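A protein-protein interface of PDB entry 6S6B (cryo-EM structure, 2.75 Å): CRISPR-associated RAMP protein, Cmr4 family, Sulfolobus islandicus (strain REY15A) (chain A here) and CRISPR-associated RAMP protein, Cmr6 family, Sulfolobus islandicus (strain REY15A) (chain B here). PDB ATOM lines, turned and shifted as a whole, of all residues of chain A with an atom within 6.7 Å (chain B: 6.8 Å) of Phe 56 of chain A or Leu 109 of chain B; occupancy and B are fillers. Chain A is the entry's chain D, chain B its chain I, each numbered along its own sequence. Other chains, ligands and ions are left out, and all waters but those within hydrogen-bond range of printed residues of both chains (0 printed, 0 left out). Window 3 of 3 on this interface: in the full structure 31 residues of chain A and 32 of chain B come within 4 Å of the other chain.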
ATOM      1  N   LYS A  50     -10.465 -11.255 -29.306  1.00  0.00           N
ATOM      2  CA  LYS A  50     -11.877 -11.602 -29.325  1.00  0.00           C
ATOM      3  C   LYS A  50     -12.178 -12.726 -28.352  1.00  0.00           C
ATOM      4  O   LYS A  50     -13.169 -12.672 -27.621  1.00  0.00           O
ATOM      5  CB  LYS A  50     -12.299 -11.992 -30.734  1.00  0.00           C
ATOM      6  CG  LYS A  50     -13.776 -12.174 -30.883  1.00  0.00           C
ATOM      7  CD  LYS A  50     -14.099 -12.596 -32.279  1.00  0.00           C
ATOM      8  CE  LYS A  50     -15.562 -12.855 -32.414  1.00  0.00           C
ATOM      9  NZ  LYS A  50     -15.875 -13.459 -33.725  1.00  0.00           N
ATOM     10  N   GLY A  51     -11.331 -13.752 -28.324  1.00  0.00           N
ATOM     11  CA  GLY A  51     -11.583 -14.871 -27.437  1.00  0.00           C
ATOM     12  C   GLY A  51     -11.617 -14.460 -25.982  1.00  0.00           C
ATOM     13  O   GLY A  51     -12.482 -14.899 -25.223  1.00  0.00           O
ATOM     14  N   ALA A  52     -10.684 -13.604 -25.576  1.00  0.00           N
ATOM     15  CA  ALA A  52     -10.604 -13.204 -24.178  1.00  0.00           C
ATOM     16  C   ALA A  52     -11.734 -12.257 -23.812  1.00  0.00           C
ATOM     17  O   ALA A  52     -12.345 -12.388 -22.746  1.00  0.00           O
ATOM     18  CB  ALA A  52      -9.252 -12.556 -23.904  1.00  0.00           C
ATOM     19  N   ILE A  53     -12.028 -11.293 -24.681  1.00  0.00           N
ATOM     20  CA  ILE A  53     -13.061 -10.318 -24.366  1.00  0.00           C
ATOM     21  C   ILE A  53     -14.438 -10.953 -24.416  1.00  0.00           C
ATOM     22  O   ILE A  53     -15.292 -10.659 -23.576  1.00  0.00           O
ATOM     23  CB  ILE A  53     -12.955  -9.115 -25.315  1.00  0.00           C
ATOM     24  CG1 ILE A  53     -11.651  -8.369 -25.057  1.00  0.00           C
ATOM     25  CG2 ILE A  53     -14.130  -8.193 -25.134  1.00  0.00           C
ATOM     26  CD1 ILE A  53     -11.428  -7.205 -25.964  1.00  0.00           C
ATOM     27  N   LYS A  54     -14.679 -11.837 -25.379  1.00  0.00           N
ATOM     28  CA  LYS A  54     -15.983 -12.479 -25.482  1.00  0.00           C
ATOM     29  C   LYS A  54     -16.252 -13.376 -24.284  1.00  0.00           C
ATOM     30  O   LYS A  54     -17.291 -13.252 -23.631  1.00  0.00           O
ATOM     31  CB  LYS A  54     -16.069 -13.277 -26.779  1.00  0.00           C
ATOM     32  CG  LYS A  54     -17.420 -13.890 -27.074  1.00  0.00           C
ATOM     33  CD  LYS A  54     -17.303 -14.808 -28.268  1.00  0.00           C
ATOM     34  CE  LYS A  54     -18.616 -15.451 -28.615  1.00  0.00           C
ATOM     35  NZ  LYS A  54     -18.482 -16.250 -29.855  1.00  0.00           N
ATOM     36  N   SER A  55     -15.323 -14.283 -23.984  1.00  0.00           N
ATOM     37  CA  SER A  55     -15.486 -15.176 -22.843  1.00  0.00           C
ATOM     38  C   SER A  55     -15.708 -14.389 -21.565  1.00  0.00           C
ATOM     39  O   SER A  55     -16.572 -14.727 -20.751  1.00  0.00           O
ATOM     40  CB  SER A  55     -14.257 -16.068 -22.705  1.00  0.00           C
ATOM     41  OG  SER A  55     -13.099 -15.284 -22.497  1.00  0.00           O
ATOM     42  N   PHE A  56     -14.922 -13.333 -21.373  1.00  0.00           N
ATOM     43  CA  PHE A  56     -15.091 -12.482 -20.207  1.00  0.00           C
ATOM     44  C   PHE A  56     -16.460 -11.825 -20.201  1.00  0.00           C
ATOM     45  O   PHE A  56     -17.133 -11.778 -19.167  1.00  0.00           O
ATOM     46  CB  PHE A  56     -13.992 -11.425 -20.183  1.00  0.00           C
ATOM     47  CG  PHE A  56     -14.169 -10.410 -19.109  1.00  0.00           C
ATOM     48  CD1 PHE A  56     -13.739 -10.668 -17.825  1.00  0.00           C
ATOM     49  CD2 PHE A  56     -14.762  -9.197 -19.380  1.00  0.00           C
ATOM     50  CE1 PHE A  56     -13.902  -9.739 -16.836  1.00  0.00           C
ATOM     51  CE2 PHE A  56     -14.926  -8.266 -18.392  1.00  0.00           C
ATOM     52  CZ  PHE A  56     -14.496  -8.537 -17.119  1.00  0.00           C
ATOM     53  N   LEU A  57     -16.884 -11.299 -21.348  1.00  0.00           N
ATOM     54  CA  LEU A  57     -18.157 -10.591 -21.410  1.00  0.00           C
ATOM     55  C   LEU A  57     -19.319 -11.514 -21.087  1.00  0.00           C
ATOM     56  O   LEU A  57     -20.272 -11.110 -20.414  1.00  0.00           O
ATOM     57  CB  LEU A  57     -18.341  -9.968 -22.789  1.00  0.00           C
ATOM     58  CG  LEU A  57     -17.663  -8.618 -22.979  1.00  0.00           C
ATOM     59  CD1 LEU A  57     -17.880  -8.102 -24.386  1.00  0.00           C
ATOM     60  CD2 LEU A  57     -18.187  -7.641 -21.952  1.00  0.00           C
ATOM     61  N   LEU A  58     -19.257 -12.759 -21.550  1.00  0.00           N
ATOM     62  CA  LEU A  58     -20.330 -13.708 -21.293  1.00  0.00           C
ATOM     63  C   LEU A  58     -20.471 -14.057 -19.821  1.00  0.00           C
ATOM     64  O   LEU A  58     -21.421 -14.754 -19.458  1.00  0.00           O
ATOM     65  CB  LEU A  58     -20.100 -14.976 -22.107  1.00  0.00           C
ATOM     66  CG  LEU A  58     -20.284 -14.799 -23.610  1.00  0.00           C
ATOM     67  CD1 LEU A  58     -19.760 -16.004 -24.353  1.00  0.00           C
ATOM     68  CD2 LEU A  58     -21.745 -14.569 -23.923  1.00  0.00           C
ATOM     69  N   LYS A  59     -19.557 -13.600 -18.973  1.00  0.00           N
ATOM     70  CA  LYS A  59     -19.658 -13.783 -17.532  1.00  0.00           C
ATOM     71  C   LYS A  59     -20.015 -12.510 -16.789  1.00  0.00           C
ATOM     72  O   LYS A  59     -20.791 -12.560 -15.837  1.00  0.00           O
ATOM     73  CB  LYS A  59     -18.344 -14.335 -16.978  1.00  0.00           C
ATOM     74  CG  LYS A  59     -17.904 -15.629 -17.620  1.00  0.00           C
ATOM     75  CD  LYS A  59     -16.613 -16.122 -17.002  1.00  0.00           C
ATOM     76  CE  LYS A  59     -16.070 -17.320 -17.750  1.00  0.00           C
ATOM     77  NZ  LYS A  59     -14.943 -17.955 -17.020  1.00  0.00           N
ATOM     78  N   GLU A  60     -19.469 -11.363 -17.198  1.00  0.00           N
ATOM     79  CA  GLU A  60     -19.815 -10.117 -16.526  1.00  0.00           C
ATOM     80  C   GLU A  60     -21.251  -9.706 -16.808  1.00  0.00           C
ATOM     81  O   GLU A  60     -21.904  -9.115 -15.942  1.00  0.00           O
ATOM     82  CB  GLU A  60     -18.871  -8.993 -16.946  1.00  0.00           C
ATOM     83  CG  GLU A  60     -19.138  -7.688 -16.201  1.00  0.00           C
ATOM     84  CD  GLU A  60     -18.242  -6.543 -16.641  1.00  0.00           C
ATOM     85  OE1 GLU A  60     -17.055  -6.787 -16.927  1.00  0.00           O
ATOM     86  OE2 GLU A  60     -18.724  -5.394 -16.691  1.00  0.00           O
ATOM     87  N   PHE A  61     -21.765 -10.009 -17.998  1.00  0.00           N
ATOM     88  CA  PHE A  61     -23.112  -9.621 -18.405  1.00  0.00           C
ATOM     89  C   PHE A  61     -23.923 -10.860 -18.765  1.00  0.00           C
ATOM     90  O   PHE A  61     -24.185 -11.116 -19.947  1.00  0.00           O
ATOM     91  CB  PHE A  61     -23.084  -8.660 -19.590  1.00  0.00           C
ATOM     92  CG  PHE A  61     -22.304  -7.405 -19.345  1.00  0.00           C
ATOM     93  CD1 PHE A  61     -20.931  -7.388 -19.484  1.00  0.00           C
ATOM     94  CD2 PHE A  61     -22.950  -6.237 -19.000  1.00  0.00           C
ATOM     95  CE1 PHE A  61     -20.216  -6.232 -19.272  1.00  0.00           C
ATOM     96  CE2 PHE A  61     -22.238  -5.079 -18.786  1.00  0.00           C
ATOM     97  CZ  PHE A  61     -20.869  -5.078 -18.920  1.00  0.00           C
ATOM     98  N   ASN A 260     -19.158  -0.233 -19.807  1.00  0.00           N
ATOM     99  CA  ASN A 260     -18.862  -0.975 -18.586  1.00  0.00           C
ATOM    100  C   ASN A 260     -17.841  -2.075 -18.838  1.00  0.00           C
ATOM    101  O   ASN A 260     -18.032  -3.228 -18.467  1.00  0.00           O
ATOM    102  CB  ASN A 260     -20.149  -1.548 -18.017  1.00  0.00           C
ATOM    103  CG  ASN A 260     -21.084  -0.481 -17.522  1.00  0.00           C
ATOM    104  OD1 ASN A 260     -20.661   0.479 -16.883  1.00  0.00           O
ATOM    105  ND2 ASN A 260     -22.366  -0.633 -17.822  1.00  0.00           N
ATOM    106  N   LEU A 261     -16.734  -1.718 -19.479  1.00  0.00           N
ATOM    107  CA  LEU A 261     -15.702  -2.694 -19.809  1.00  0.00           C
ATOM    108  C   LEU A 261     -14.359  -1.991 -19.663  1.00  0.00           C
ATOM    109  O   LEU A 261     -13.960  -1.227 -20.545  1.00  0.00           O
ATOM    110  CB  LEU A 261     -15.897  -3.246 -21.211  1.00  0.00           C
ATOM    111  CG  LEU A 261     -14.953  -4.373 -21.627  1.00  0.00           C
ATOM    112  CD1 LEU A 261     -15.245  -5.627 -20.838  1.00  0.00           C
ATOM    113  CD2 LEU A 261     -15.077  -4.641 -23.107  1.00  0.00           C
ATOM    114  N   ARG A 262     -13.679  -2.244 -18.558  1.00  0.00           N
ATOM    115  CA  ARG A 262     -12.394  -1.612 -18.306  1.00  0.00           C
ATOM    116  C   ARG A 262     -11.261  -2.600 -18.102  1.00  0.00           C
ATOM    117  O   ARG A 262     -10.153  -2.358 -18.580  1.00  0.00           O
ATOM    118  CB  ARG A 262     -12.487  -0.693 -17.087  1.00  0.00           C
ATOM    119  CG  ARG A 262     -11.316   0.251 -16.962  1.00  0.00           C
ATOM    120  CD  ARG A 262     -11.749   1.579 -16.413  1.00  0.00           C
ATOM    121  NE  ARG A 262     -12.338   1.441 -15.091  1.00  0.00           N
ATOM    122  CZ  ARG A 262     -11.710   1.748 -13.964  1.00  0.00           C
ATOM    123  NH1 ARG A 262     -10.468   2.211 -14.005  1.00  0.00           N
ATOM    124  NH2 ARG A 262     -12.322   1.594 -12.798  1.00  0.00           N
ATOM    125  N   TYR A 263     -11.501  -3.706 -17.406  1.00  0.00           N
ATOM    126  CA  TYR A 263     -10.454  -4.658 -17.071  1.00  0.00           C
ATOM    127  C   TYR A 263     -10.805  -6.020 -17.641  1.00  0.00           C
ATOM    128  O   TYR A 263     -11.936  -6.488 -17.487  1.00  0.00           O
ATOM    129  CB  TYR A 263     -10.264  -4.746 -15.560  1.00  0.00           C
ATOM    130  CG  TYR A 263      -9.889  -3.432 -14.935  1.00  0.00           C
ATOM    131  CD1 TYR A 263      -8.679  -2.830 -15.224  1.00  0.00           C
ATOM    132  CD2 TYR A 263     -10.747  -2.789 -14.065  1.00  0.00           C
ATOM    133  CE1 TYR A 263      -8.334  -1.630 -14.659  1.00  0.00           C
ATOM    134  CE2 TYR A 263     -10.410  -1.590 -13.498  1.00  0.00           C
ATOM    135  CZ  TYR A 263      -9.204  -1.015 -13.798  1.00  0.00           C
ATOM    136  OH  TYR A 263      -8.863   0.187 -13.229  1.00  0.00           O
ATOM    137  N   VAL A 264      -9.829  -6.653 -18.289  1.00  0.00           N
ATOM    138  CA  VAL A 264     -10.010  -7.939 -18.950  1.00  0.00           C
ATOM    139  C   VAL A 264      -8.729  -8.734 -18.746  1.00  0.00           C
ATOM    140  O   VAL A 264      -7.658  -8.163 -18.544  1.00  0.00           O
ATOM    141  CB  VAL A 264     -10.338  -7.756 -20.454  1.00  0.00           C
ATOM    142  CG1 VAL A 264     -10.378  -9.077 -21.179  1.00  0.00           C
ATOM    143  CG2 VAL A 264     -11.665  -7.059 -20.633  1.00  0.00           C
ATOM    144  N   ILE A 265      -8.841 -10.058 -18.775  1.00  0.00           N
ATOM    145  CA  ILE A 265      -7.691 -10.947 -18.660  1.00  0.00           C
ATOM    146  C   ILE A 265      -7.424 -11.560 -20.028  1.00  0.00           C
ATOM    147  O   ILE A 265      -8.289 -12.241 -20.589  1.00  0.00           O
ATOM    148  CB  ILE A 265      -7.922 -12.029 -17.600  1.00  0.00           C
ATOM    149  CG1 ILE A 265      -8.194 -11.379 -16.249  1.00  0.00           C
ATOM    150  CG2 ILE A 265      -6.726 -12.941 -17.511  1.00  0.00           C
ATOM    151  CD1 ILE A 265      -8.528 -12.357 -15.164  1.00  0.00           C
ATOM    152  N   ILE A 276      -3.763  -9.711 -16.708  1.00  0.00           N
ATOM    153  CA  ILE A 276      -4.661  -8.616 -16.372  1.00  0.00           C
ATOM    154  C   ILE A 276      -4.280  -7.399 -17.196  1.00  0.00           C
ATOM    155  O   ILE A 276      -3.097  -7.063 -17.326  1.00  0.00           O
ATOM    156  CB  ILE A 276      -4.616  -8.306 -14.871  1.00  0.00           C
ATOM    157  CG1 ILE A 276      -4.968  -9.552 -14.067  1.00  0.00           C
ATOM    158  CG2 ILE A 276      -5.580  -7.193 -14.542  1.00  0.00           C
ATOM    159  CD1 ILE A 276      -4.365  -9.561 -12.693  1.00  0.00           C
ATOM    160  N   VAL A 277      -5.280  -6.736 -17.768  1.00  0.00           N
ATOM    161  CA  VAL A 277      -5.037  -5.674 -18.730  1.00  0.00           C
ATOM    162  C   VAL A 277      -6.192  -4.693 -18.638  1.00  0.00           C
ATOM    163  O   VAL A 277      -7.263  -5.013 -18.126  1.00  0.00           O
ATOM    164  CB  VAL A 277      -4.900  -6.240 -20.160  1.00  0.00           C
ATOM    165  CG1 VAL A 277      -6.262  -6.439 -20.784  1.00  0.00           C
ATOM    166  CG2 VAL A 277      -4.006  -5.388 -20.993  1.00  0.00           C
ATOM    167  N   GLU B 104      -7.625  -3.145  -6.145  1.00  0.00           N
ATOM    168  CA  GLU B 104      -8.909  -2.562  -6.511  1.00  0.00           C
ATOM    169  C   GLU B 104      -9.400  -3.115  -7.839  1.00  0.00           C
ATOM    170  O   GLU B 104     -10.602  -3.318  -8.028  1.00  0.00           O
ATOM    171  CB  GLU B 104      -8.795  -1.043  -6.569  1.00  0.00           C
ATOM    172  CG  GLU B 104     -10.061  -0.350  -7.026  1.00  0.00           C
ATOM    173  CD  GLU B 104     -11.091  -0.211  -5.922  1.00  0.00           C
ATOM    174  OE1 GLU B 104     -10.894  -0.793  -4.836  1.00  0.00           O
ATOM    175  OE2 GLU B 104     -12.102   0.490  -6.143  1.00  0.00           O
ATOM    176  N   VAL B 105      -8.479  -3.364  -8.770  1.00  0.00           N
ATOM    177  CA  VAL B 105      -8.846  -3.975 -10.043  1.00  0.00           C
ATOM    178  C   VAL B 105      -9.483  -5.337  -9.812  1.00  0.00           C
ATOM    179  O   VAL B 105     -10.544  -5.649 -10.362  1.00  0.00           O
ATOM    180  CB  VAL B 105      -7.613  -4.086 -10.954  1.00  0.00           C
ATOM    181  CG1 VAL B 105      -7.907  -4.988 -12.126  1.00  0.00           C
ATOM    182  CG2 VAL B 105      -7.173  -2.716 -11.414  1.00  0.00           C
ATOM    183  N   LEU B 106      -8.845  -6.168  -8.988  1.00  0.00           N
ATOM    184  CA  LEU B 106      -9.351  -7.514  -8.761  1.00  0.00           C
ATOM    185  C   LEU B 106     -10.686  -7.499  -8.035  1.00  0.00           C
ATOM    186  O   LEU B 106     -11.466  -8.445  -8.165  1.00  0.00           O
ATOM    187  CB  LEU B 106      -8.333  -8.330  -7.975  1.00  0.00           C
ATOM    188  CG  LEU B 106      -6.932  -8.379  -8.575  1.00  0.00           C
ATOM    189  CD1 LEU B 106      -5.978  -9.063  -7.626  1.00  0.00           C
ATOM    190  CD2 LEU B 106      -6.956  -9.091  -9.903  1.00  0.00           C
ATOM    191  N   LYS B 107     -10.965  -6.448  -7.264  1.00  0.00           N
ATOM    192  CA  LYS B 107     -12.294  -6.319  -6.680  1.00  0.00           C
ATOM    193  C   LYS B 107     -13.322  -5.992  -7.750  1.00  0.00           C
ATOM    194  O   LYS B 107     -14.427  -6.544  -7.747  1.00  0.00           O
ATOM    195  CB  LYS B 107     -12.293  -5.250  -5.592  1.00  0.00           C
ATOM    196  CG  LYS B 107     -12.146  -5.797  -4.190  1.00  0.00           C
ATOM    197  CD  LYS B 107     -12.079  -4.675  -3.175  1.00  0.00           C
ATOM    198  CE  LYS B 107     -10.942  -3.719  -3.493  1.00  0.00           C
ATOM    199  NZ  LYS B 107     -11.006  -2.470  -2.690  1.00  0.00           N
ATOM    200  N   SER B 108     -12.974  -5.089  -8.667  1.00  0.00           N
ATOM    201  CA  SER B 108     -13.823  -4.831  -9.822  1.00  0.00           C
ATOM    202  C   SER B 108     -14.150  -6.119 -10.563  1.00  0.00           C
ATOM    203  O   SER B 108     -15.293  -6.335 -10.977  1.00  0.00           O
ATOM    204  CB  SER B 108     -13.137  -3.834 -10.753  1.00  0.00           C
ATOM    205  OG  SER B 108     -13.905  -3.605 -11.918  1.00  0.00           O
ATOM    206  N   LEU B 109     -13.160  -6.993 -10.732  1.00  0.00           N
ATOM    207  CA  LEU B 109     -13.375  -8.287 -11.361  1.00  0.00           C
ATOM    208  C   LEU B 109     -14.026  -9.295 -10.428  1.00  0.00           C
ATOM    209  O   LEU B 109     -14.232 -10.442 -10.836  1.00  0.00           O
ATOM    210  CB  LEU B 109     -12.049  -8.847 -11.876  1.00  0.00           C
ATOM    211  CG  LEU B 109     -11.390  -8.072 -13.018  1.00  0.00           C
ATOM    212  CD1 LEU B 109      -9.999  -8.593 -13.302  1.00  0.00           C
ATOM    213  CD2 LEU B 109     -12.238  -8.148 -14.257  1.00  0.00           C
ATOM    214  N   LYS B 110     -14.329  -8.902  -9.189  1.00  0.00           N
ATOM    215  CA  LYS B 110     -15.101  -9.717  -8.249  1.00  0.00           C
ATOM    216  C   LYS B 110     -14.342 -10.968  -7.811  1.00  0.00           C
ATOM    217  O   LYS B 110     -14.910 -12.055  -7.729  1.00  0.00           O
ATOM    218  CB  LYS B 110     -16.466 -10.085  -8.830  1.00  0.00           C
ATOM    219  CG  LYS B 110     -17.324  -8.883  -9.136  1.00  0.00           C
ATOM    220  CD  LYS B 110     -18.199  -9.120 -10.342  1.00  0.00           C
ATOM    221  CE  LYS B 110     -19.037  -7.890 -10.639  1.00  0.00           C
ATOM    222  NZ  LYS B 110     -18.214  -6.649 -10.667  1.00  0.00           N
ATOM    223  N   TYR B 111     -13.058 -10.816  -7.520  1.00  0.00           N
ATOM    224  CA  TYR B 111     -12.291 -11.885  -6.906  1.00  0.00           C
ATOM    225  C   TYR B 111     -12.321 -11.744  -5.391  1.00  0.00           C
ATOM    226  O   TYR B 111     -12.751 -10.729  -4.844  1.00  0.00           O
ATOM    227  CB  TYR B 111     -10.849 -11.866  -7.398  1.00  0.00           C
ATOM    228  CG  TYR B 111     -10.650 -12.471  -8.760  1.00  0.00           C
ATOM    229  CD1 TYR B 111     -10.548 -13.837  -8.920  1.00  0.00           C
ATOM    230  CD2 TYR B 111     -10.549 -11.672  -9.883  1.00  0.00           C
ATOM    231  CE1 TYR B 111     -10.361 -14.391 -10.155  1.00  0.00           C
ATOM    232  CE2 TYR B 111     -10.364 -12.219 -11.125  1.00  0.00           C
ATOM    233  CZ  TYR B 111     -10.270 -13.580 -11.255  1.00  0.00           C
ATOM    234  OH  TYR B 111     -10.084 -14.136 -12.496  1.00  0.00           O
ATOM    235  N   LYS B 243     -11.891 -17.459  -7.020  1.00  0.00           N
ATOM    236  CA  LYS B 243     -13.330 -17.264  -7.048  1.00  0.00           C
ATOM    237  C   LYS B 243     -14.104 -18.242  -6.183  1.00  0.00           C
ATOM    238  O   LYS B 243     -15.159 -17.875  -5.667  1.00  0.00           O
ATOM    239  CB  LYS B 243     -13.854 -17.351  -8.486  1.00  0.00           C
ATOM    240  CG  LYS B 243     -13.449 -16.175  -9.339  1.00  0.00           C
ATOM    241  CD  LYS B 243     -14.036 -16.279 -10.725  1.00  0.00           C
ATOM    242  CE  LYS B 243     -13.622 -15.095 -11.572  1.00  0.00           C
ATOM    243  NZ  LYS B 243     -14.235 -13.843 -11.059  1.00  0.00           N
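Phe 56 of chain A touches just one residue of chain B: Leu 109 (3.5 Å).
Asn 260 of chain A touches none of the printed residues of chain B.
Of the printed residues of chain B, Tyr 263 of chain A touches Val 105, Ser 108 and Leu 109.
Of the printed residues of chain B, Ile 276 of chain A touches Leu 106 (3.8 Å).
Of the printed residues of chain A, Leu 106 of chain B touches Ile 276 (3.8 Å).
Leu 109 of chain B touches two residues of chain A.
The nearest residue of chain B that does not touch Phe 56 of chain A is Ser 108 of chain B (6.6 Å).
Among the printed residues, pairs that only touch across the chains: Phe 56 of chain A with Leu 109 of chain B (3.5 Å), Tyr 263 of chain A with Val 105 of chain B (3.6 Å), Ile 265 of chain A with Tyr 111 of chain B (3.6 Å), Tyr 263 of chain A with Leu 109 of chain B (3.6 Å), Ile 276 of chain A with Leu 106 of chain B (3.8 Å) and Tyr 263 of chain A with Ser 108 of chain B (3.9 Å).
The backbone carbonyl oxygen (O) of Ser 108 of chain B sits at hydrogen-bond distance from the side-chain amino group (NZ) of Lys 110 of chain B (3.0 Å).
The side-chain amino group of Lys 243 of chain B is in hydrogen-bond range of the backbone carbonyl oxygen of Leu 109 of chain B, 3.4 Å away.
OH of Tyr 263 of chain A is in hydrogen-bond range of NH1 of Arg 262 of chain A, at 2.7 Å.
The backbone carbonyl oxygen of Leu 106 of chain B lies within hydrogen-bond range of the backbone NH of Tyr 111 of chain B, 2.9 Å away.
Hydrophobic or aromatic side chains of chain A that line the printed part of chain B: Phe 56, Tyr 263, Ile 265 and Ile 276.
Hydrophobic or aromatic side chains of chain B that line the printed part of chain A: Val 105, Leu 106, Leu 109 and Tyr 111.
Along chain B the printed residues that touch a printed residue of chain A span positions 105 to 111.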
